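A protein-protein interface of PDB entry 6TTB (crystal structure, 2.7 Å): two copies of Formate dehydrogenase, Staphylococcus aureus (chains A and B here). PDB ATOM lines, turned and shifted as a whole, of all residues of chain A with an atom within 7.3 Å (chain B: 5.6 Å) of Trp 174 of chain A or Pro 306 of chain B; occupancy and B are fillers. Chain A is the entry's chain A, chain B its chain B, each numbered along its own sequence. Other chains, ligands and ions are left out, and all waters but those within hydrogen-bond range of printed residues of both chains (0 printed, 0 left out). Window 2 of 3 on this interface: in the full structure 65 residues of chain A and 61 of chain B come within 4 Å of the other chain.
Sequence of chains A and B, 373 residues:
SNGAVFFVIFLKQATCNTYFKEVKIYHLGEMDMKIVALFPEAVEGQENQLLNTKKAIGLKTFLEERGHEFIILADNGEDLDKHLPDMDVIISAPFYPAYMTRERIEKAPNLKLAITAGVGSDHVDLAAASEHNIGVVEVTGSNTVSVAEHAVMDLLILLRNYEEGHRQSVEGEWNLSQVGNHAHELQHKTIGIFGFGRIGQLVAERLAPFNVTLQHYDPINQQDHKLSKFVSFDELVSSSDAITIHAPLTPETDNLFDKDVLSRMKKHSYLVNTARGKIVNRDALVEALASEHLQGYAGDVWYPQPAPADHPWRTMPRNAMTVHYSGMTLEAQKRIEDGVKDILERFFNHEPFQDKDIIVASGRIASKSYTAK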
ATOM      1  N   GLN A 168      33.567 -14.187 -20.930  1.00  0.00           N
ATOM      2  CA  GLN A 168      33.128 -14.039 -19.566  1.00  0.00           C
ATOM      3  C   GLN A 168      33.016 -15.408 -18.920  1.00  0.00           C
ATOM      4  O   GLN A 168      33.500 -15.578 -17.808  1.00  0.00           O
ATOM      5  CB  GLN A 168      31.789 -13.291 -19.493  1.00  0.00           C
ATOM      6  CG  GLN A 168      31.847 -11.757 -19.544  1.00  0.00           C
ATOM      7  CD  GLN A 168      30.474 -11.234 -19.192  1.00  0.00           C
ATOM      8  OE1 GLN A 168      29.738 -11.881 -18.470  1.00  0.00           O
ATOM      9  NE2 GLN A 168      30.068 -10.103 -19.757  1.00  0.00           N
ATOM     10  N   SER A 169      32.328 -16.374 -19.568  1.00  0.00           N
ATOM     11  CA  SER A 169      32.258 -17.718 -18.974  1.00  0.00           C
ATOM     12  C   SER A 169      33.669 -18.175 -18.604  1.00  0.00           C
ATOM     13  O   SER A 169      34.021 -18.324 -17.417  1.00  0.00           O
ATOM     14  CB  SER A 169      31.606 -18.716 -19.899  1.00  0.00           C
ATOM     15  OG  SER A 169      31.817 -20.091 -19.476  1.00  0.00           O
ATOM     16  N   GLU A 171      36.552 -16.583 -18.464  1.00  0.00           N
ATOM     17  CA  GLU A 171      37.564 -15.766 -17.797  1.00  0.00           C
ATOM     18  C   GLU A 171      37.173 -15.471 -16.334  1.00  0.00           C
ATOM     19  O   GLU A 171      37.846 -14.712 -15.649  1.00  0.00           O
ATOM     20  CB  GLU A 171      37.937 -14.545 -18.648  1.00  0.00           C
ATOM     21  CG  GLU A 171      39.032 -14.878 -19.637  1.00  0.00           C
ATOM     22  CD  GLU A 171      39.214 -13.924 -20.832  1.00  0.00           C
ATOM     23  OE1 GLU A 171      39.420 -12.657 -20.622  1.00  0.00           O
ATOM     24  OE2 GLU A 171      39.183 -14.429 -21.990  1.00  0.00           O
ATOM     25  N   GLY A 172      36.152 -16.160 -15.819  1.00  0.00           N
ATOM     26  CA  GLY A 172      35.817 -16.068 -14.402  1.00  0.00           C
ATOM     27  C   GLY A 172      34.684 -15.080 -14.137  1.00  0.00           C
ATOM     28  O   GLY A 172      34.265 -14.889 -12.993  1.00  0.00           O
ATOM     29  N   GLU A 173      34.137 -14.519 -15.212  1.00  0.00           N
ATOM     30  CA  GLU A 173      33.330 -13.319 -15.137  1.00  0.00           C
ATOM     31  C   GLU A 173      31.817 -13.598 -15.107  1.00  0.00           C
ATOM     32  O   GLU A 173      31.364 -14.742 -15.277  1.00  0.00           O
ATOM     33  CB  GLU A 173      33.660 -12.473 -16.320  1.00  0.00           C
ATOM     34  CG  GLU A 173      34.950 -11.780 -16.114  1.00  0.00           C
ATOM     35  CD  GLU A 173      35.273 -10.830 -17.251  1.00  0.00           C
ATOM     36  OE1 GLU A 173      36.397 -10.349 -17.271  1.00  0.00           O
ATOM     37  OE2 GLU A 173      34.371 -10.585 -18.134  1.00  0.00           O
ATOM     38  N   TRP A 174      31.058 -12.517 -14.842  1.00  0.00           N
ATOM     39  CA  TRP A 174      29.614 -12.540 -14.886  1.00  0.00           C
ATOM     40  C   TRP A 174      29.048 -11.118 -14.880  1.00  0.00           C
ATOM     41  O   TRP A 174      28.746 -10.573 -13.841  1.00  0.00           O
ATOM     42  CB  TRP A 174      29.020 -13.436 -13.783  1.00  0.00           C
ATOM     43  CG  TRP A 174      27.536 -13.682 -13.941  1.00  0.00           C
ATOM     44  CD1 TRP A 174      26.530 -12.816 -13.607  1.00  0.00           C
ATOM     45  CD2 TRP A 174      26.880 -14.874 -14.442  1.00  0.00           C
ATOM     46  NE1 TRP A 174      25.313 -13.375 -13.883  1.00  0.00           N
ATOM     47  CE2 TRP A 174      25.492 -14.656 -14.339  1.00  0.00           C
ATOM     48  CE3 TRP A 174      27.316 -16.127 -14.876  1.00  0.00           C
ATOM     49  CZ2 TRP A 174      24.554 -15.604 -14.727  1.00  0.00           C
ATOM     50  CZ3 TRP A 174      26.387 -17.076 -15.228  1.00  0.00           C
ATOM     51  CH2 TRP A 174      25.026 -16.796 -15.197  1.00  0.00           C
ATOM     52  N   ASN A 175      28.843 -10.551 -16.078  1.00  0.00           N
ATOM     53  CA  ASN A 175      28.624  -9.128 -16.245  1.00  0.00           C
ATOM     54  C   ASN A 175      27.678  -8.936 -17.397  1.00  0.00           C
ATOM     55  O   ASN A 175      28.089  -8.918 -18.540  1.00  0.00           O
ATOM     56  CB  ASN A 175      29.902  -8.345 -16.535  1.00  0.00           C
ATOM     57  CG  ASN A 175      29.595  -6.889 -16.813  1.00  0.00           C
ATOM     58  OD1 ASN A 175      28.488  -6.416 -16.527  1.00  0.00           O
ATOM     59  ND2 ASN A 175      30.542  -6.170 -17.412  1.00  0.00           N
ATOM     60  N   LEU A 176      26.422  -8.721 -17.073  1.00  0.00           N
ATOM     61  CA  LEU A 176      25.382  -8.788 -18.069  1.00  0.00           C
ATOM     62  C   LEU A 176      25.274  -7.469 -18.833  1.00  0.00           C
ATOM     63  O   LEU A 176      24.664  -7.405 -19.880  1.00  0.00           O
ATOM     64  CB  LEU A 176      24.087  -9.190 -17.365  1.00  0.00           C
ATOM     65  CG  LEU A 176      23.814 -10.697 -17.423  1.00  0.00           C
ATOM     66  CD1 LEU A 176      25.106 -11.493 -17.345  1.00  0.00           C
ATOM     67  CD2 LEU A 176      22.846 -11.141 -16.348  1.00  0.00           C
ATOM     68  N   SER A 177      25.831  -6.403 -18.291  1.00  0.00           N
ATOM     69  CA  SER A 177      25.750  -5.139 -19.008  1.00  0.00           C
ATOM     70  C   SER A 177      26.558  -5.259 -20.276  1.00  0.00           C
ATOM     71  O   SER A 177      26.115  -4.826 -21.337  1.00  0.00           O
ATOM     72  CB  SER A 177      26.218  -3.984 -18.180  1.00  0.00           C
ATOM     73  OG  SER A 177      25.218  -3.694 -17.203  1.00  0.00           O
ATOM     74  N   VAL A 179      27.862  -7.925 -21.891  1.00  0.00           N
ATOM     75  CA  VAL A 179      27.394  -8.874 -22.885  1.00  0.00           C
ATOM     76  C   VAL A 179      26.159  -8.291 -23.511  1.00  0.00           C
ATOM     77  O   VAL A 179      25.963  -8.360 -24.740  1.00  0.00           O
ATOM     78  CB  VAL A 179      26.976 -10.227 -22.338  1.00  0.00           C
ATOM     79  CG1 VAL A 179      27.330 -11.347 -23.287  1.00  0.00           C
ATOM     80  CG2 VAL A 179      27.340 -10.491 -20.879  1.00  0.00           C
ATOM     81  N   ASP B 300      23.736 -22.171 -21.143  1.00  0.00           N
ATOM     82  CA  ASP B 300      23.924 -20.879 -20.492  1.00  0.00           C
ATOM     83  C   ASP B 300      23.255 -20.857 -19.106  1.00  0.00           C
ATOM     84  O   ASP B 300      22.992 -19.786 -18.574  1.00  0.00           O
ATOM     85  CB  ASP B 300      23.461 -19.738 -21.392  1.00  0.00           C
ATOM     86  CG  ASP B 300      21.945 -19.685 -21.513  1.00  0.00           C
ATOM     87  OD1 ASP B 300      21.297 -20.759 -21.313  1.00  0.00           O
ATOM     88  OD2 ASP B 300      21.403 -18.557 -21.799  1.00  0.00           O
ATOM     89  N   TRP B 302      23.209 -22.513 -14.984  1.00  0.00           N
ATOM     90  CA  TRP B 302      24.237 -22.968 -14.062  1.00  0.00           C
ATOM     91  C   TRP B 302      23.659 -23.350 -12.709  1.00  0.00           C
ATOM     92  O   TRP B 302      22.691 -22.733 -12.254  1.00  0.00           O
ATOM     93  CB  TRP B 302      25.313 -21.907 -13.889  1.00  0.00           C
ATOM     94  CG  TRP B 302      25.911 -21.438 -15.164  1.00  0.00           C
ATOM     95  CD1 TRP B 302      25.283 -20.753 -16.168  1.00  0.00           C
ATOM     96  CD2 TRP B 302      27.296 -21.510 -15.529  1.00  0.00           C
ATOM     97  NE1 TRP B 302      26.181 -20.415 -17.137  1.00  0.00           N
ATOM     98  CE2 TRP B 302      27.432 -20.864 -16.767  1.00  0.00           C
ATOM     99  CE3 TRP B 302      28.427 -22.045 -14.922  1.00  0.00           C
ATOM    100  CZ2 TRP B 302      28.648 -20.772 -17.426  1.00  0.00           C
ATOM    101  CZ3 TRP B 302      29.639 -21.939 -15.556  1.00  0.00           C
ATOM    102  CH2 TRP B 302      29.743 -21.320 -16.807  1.00  0.00           C
ATOM    103  N   PRO B 304      25.332 -22.851  -8.898  1.00  0.00           N
ATOM    104  CA  PRO B 304      24.131 -22.004  -8.904  1.00  0.00           C
ATOM    105  C   PRO B 304      24.333 -20.781  -9.811  1.00  0.00           C
ATOM    106  O   PRO B 304      25.350 -20.662 -10.451  1.00  0.00           O
ATOM    107  CB  PRO B 304      24.082 -21.573  -7.430  1.00  0.00           C
ATOM    108  CG  PRO B 304      25.571 -21.400  -7.062  1.00  0.00           C
ATOM    109  CD  PRO B 304      26.293 -22.504  -7.823  1.00  0.00           C
ATOM    110  N   GLN B 305      23.363 -19.860  -9.851  1.00  0.00           N
ATOM    111  CA  GLN B 305      23.458 -18.735 -10.754  1.00  0.00           C
ATOM    112  C   GLN B 305      23.166 -17.482  -9.987  1.00  0.00           C
ATOM    113  O   GLN B 305      22.075 -17.388  -9.441  1.00  0.00           O
ATOM    114  CB  GLN B 305      22.360 -18.818 -11.807  1.00  0.00           C
ATOM    115  CG  GLN B 305      22.891 -19.286 -13.169  1.00  0.00           C
ATOM    116  CD  GLN B 305      21.894 -19.325 -14.312  1.00  0.00           C
ATOM    117  OE1 GLN B 305      21.759 -20.330 -15.007  1.00  0.00           O
ATOM    118  NE2 GLN B 305      21.294 -18.194 -14.605  1.00  0.00           N
ATOM    119  N   PRO B 306      23.939 -16.387 -10.206  1.00  0.00           N
ATOM    120  CA  PRO B 306      25.131 -16.418 -11.038  1.00  0.00           C
ATOM    121  C   PRO B 306      26.105 -17.507 -10.652  1.00  0.00           C
ATOM    122  O   PRO B 306      26.311 -17.745  -9.498  1.00  0.00           O
ATOM    123  CB  PRO B 306      25.833 -15.107 -10.647  1.00  0.00           C
ATOM    124  CG  PRO B 306      24.711 -14.146 -10.254  1.00  0.00           C
ATOM    125  CD  PRO B 306      23.493 -15.000  -9.955  1.00  0.00           C
ATOM    126  N   ALA B 307      26.754 -18.092 -11.654  1.00  0.00           N
ATOM    127  CA  ALA B 307      27.850 -19.013 -11.463  1.00  0.00           C
ATOM    128  C   ALA B 307      28.963 -18.360 -10.663  1.00  0.00           C
ATOM    129  O   ALA B 307      29.510 -17.322 -11.042  1.00  0.00           O
ATOM    130  CB  ALA B 307      28.356 -19.508 -12.787  1.00  0.00           C
ATOM    131  N   PRO B 308      29.338 -18.978  -9.529  1.00  0.00           N
ATOM    132  CA  PRO B 308      30.574 -18.641  -8.839  1.00  0.00           C
ATOM    133  C   PRO B 308      31.709 -18.552  -9.845  1.00  0.00           C
ATOM    134  O   PRO B 308      31.777 -19.345 -10.793  1.00  0.00           O
ATOM    135  CB  PRO B 308      30.845 -19.890  -7.982  1.00  0.00           C
ATOM    136  CG  PRO B 308      29.462 -20.501  -7.719  1.00  0.00           C
ATOM    137  CD  PRO B 308      28.601 -20.098  -8.900  1.00  0.00           C
ATOM    138  N   ARG B 314      33.235 -23.646 -16.121  1.00  0.00           N
ATOM    139  CA  ARG B 314      33.808 -22.554 -16.893  1.00  0.00           C
ATOM    140  C   ARG B 314      35.030 -23.066 -17.632  1.00  0.00           C
ATOM    141  O   ARG B 314      35.136 -22.852 -18.831  1.00  0.00           O
ATOM    142  CB  ARG B 314      34.184 -21.375 -16.004  1.00  0.00           C
ATOM    143  CG  ARG B 314      33.035 -20.798 -15.205  1.00  0.00           C
ATOM    144  CD  ARG B 314      33.512 -19.667 -14.314  1.00  0.00           C
ATOM    145  NE  ARG B 314      32.456 -18.818 -13.778  1.00  0.00           N
ATOM    146  CZ  ARG B 314      32.075 -17.632 -14.282  1.00  0.00           C
ATOM    147  NH1 ARG B 314      32.686 -17.103 -15.356  1.00  0.00           N
ATOM    148  NH2 ARG B 314      31.113 -16.953 -13.662  1.00  0.00           N
ATOM    149  N   THR B 322      28.166 -20.081 -22.030  1.00  0.00           N
ATOM    150  CA  THR B 322      28.210 -18.651 -21.778  1.00  0.00           C
ATOM    151  C   THR B 322      27.621 -18.390 -20.384  1.00  0.00           C
ATOM    152  O   THR B 322      27.009 -19.262 -19.772  1.00  0.00           O
ATOM    153  CB  THR B 322      27.429 -17.897 -22.852  1.00  0.00           C
ATOM    154  OG1 THR B 322      26.036 -18.268 -22.740  1.00  0.00           O
ATOM    155  CG2 THR B 322      27.979 -18.128 -24.249  1.00  0.00           C
ATOM    156  N   VAL B 323      27.750 -17.171 -19.890  1.00  0.00           N
ATOM    157  CA  VAL B 323      26.956 -16.780 -18.733  1.00  0.00           C
ATOM    158  C   VAL B 323      25.518 -16.648 -19.225  1.00  0.00           C
ATOM    159  O   VAL B 323      25.305 -16.650 -20.446  1.00  0.00           O
ATOM    160  CB  VAL B 323      27.489 -15.446 -18.200  1.00  0.00           C
ATOM    161  CG1 VAL B 323      28.987 -15.455 -18.061  1.00  0.00           C
ATOM    162  CG2 VAL B 323      27.117 -14.342 -19.130  1.00  0.00           C
ATOM    163  N   HIS B 324      24.537 -16.495 -18.282  1.00  0.00           N
ATOM    164  CA  HIS B 324      23.123 -16.465 -18.659  1.00  0.00           C
ATOM    165  C   HIS B 324      22.671 -15.036 -18.957  1.00  0.00           C
ATOM    166  O   HIS B 324      22.050 -14.364 -18.141  1.00  0.00           O
ATOM    167  CB  HIS B 324      22.227 -17.196 -17.640  1.00  0.00           C
ATOM    168  CG  HIS B 324      20.791 -17.325 -18.115  1.00  0.00           C
ATOM    169  ND1 HIS B 324      20.255 -18.511 -18.657  1.00  0.00           N
ATOM    170  CD2 HIS B 324      19.783 -16.424 -18.174  1.00  0.00           C
ATOM    171  CE1 HIS B 324      19.011 -18.294 -19.061  1.00  0.00           C
ATOM    172  NE2 HIS B 324      18.706 -17.034 -18.777  1.00  0.00           N
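Among the printed residues, pairs that only touch across the chains: Gly 172 of chain A with Arg 314 of chain B (3.1 Å), Trp 174 of chain A with His 324 of chain B (3.1 Å), Trp 174 of chain A with Val 323 of chain B (3.4 Å), Ser 169 of chain A with Trp 302 of chain B (3.6 Å), Gln 168 of chain A with Val 323 of chain B (3.7 Å), Trp 174 of chain A with Pro 306 of chain B (3.7 Å), Glu 173 of chain A with Val 323 of chain B (3.7 Å), Trp 174 of chain A with Ala 307 of chain B (3.7 Å), Leu 176 of chain A with His 324 of chain B (3.8 Å), Ser 169 of chain A with Val 323 of chain B (3.8 Å), Trp 174 of chain A with Trp 302 of chain B (3.9 Å), Trp 174 of chain A with Gln 305 of chain B (3.9 Å), Ser 169 of chain A with Thr 322 of chain B (3.9 Å) and Leu 176 of chain A with Val 323 of chain B (3.9 Å).
Of the printed residues of chain B, Gln 168 of chain A touches Arg 314 and Val 323.
Printed residues of chain B within 4 Å of Trp 174 of chain A: Trp 302, Gln 305, Pro 306, Ala 307, Val 323 and His 324.
Of the printed residues of chain A, Trp 302 of chain B touches Ser 169 and Trp 174.
Pro 304 of chain B touches none of the printed residues of chain A.
Pro 308 of chain B touches none of the printed residues of chain A.
Of the printed residues of chain A, Thr 322 of chain B touches Ser 169 (3.9 Å).
Of the printed residues of chain A, His 324 of chain B touches Trp 174 and Leu 176.
The nearest residue of chain B that does not touch Trp 174 of chain A is Arg 314 of chain B (4.1 Å).
The nearest residue of chain A that does not touch Pro 306 of chain B is Leu 176 of chain A (7.0 Å).
The nearest printed residue of chain B that does not touch Leu 176 of chain A is Pro 306 of chain B (7.0 Å).
The indole nitrogen (NE1) of Trp 302 of chain B lies within hydrogen-bond range of the backbone carbonyl oxygen (O) of Thr 322 of chain B.
The backbone carbonyl oxygen of Ala 307 of chain B is in hydrogen-bond range of the guanidinium group of Arg 314 of chain B.
A ring nitrogen (ND1) of His 324 of chain B lies close to the backbone carbonyl oxygen (O) of Asp 300 of chain B.
The backbone carbonyl oxygen (O) of Gln 168 of chain A sits at hydrogen-bond distance from the backbone NH (N) of Glu 173 of chain A.
NE2 of Gln 168 of chain A is in hydrogen-bond range of O of Asn 175 of chain A, at 2.6 Å.
The guanidinium group (NE) of Arg 314 of chain B sits at hydrogen-bond distance from the backbone carbonyl oxygen (O) of Pro 308 of chain B, 3.1 Å away.
Among the printed residues, no Asp or Glu carboxylate lies within 4 Å of a Lys or Arg side-chain nitrogen of the other chain.
No position is printed for both chains.
Of the 17 pairs that touch across the chains among the printed residues, none has its exchanged pair printed and touching as well.
The guanidinium group (NH1) of Arg 314 of chain B sits at hydrogen-bond distance from the backbone carbonyl oxygen (O) of Glu 173 of chain A (2.7 Å).
The guanidinium group of Arg 314 of chain B lies within hydrogen-bond range of the backbone carbonyl oxygen of Ser 169 of chain A (2.7 Å).
The guanidinium group (NH1) of Arg 314 of chain B lies within hydrogen-bond range of the backbone carbonyl oxygen (O) of Gln 168 of chain A, 3.0 Å away.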
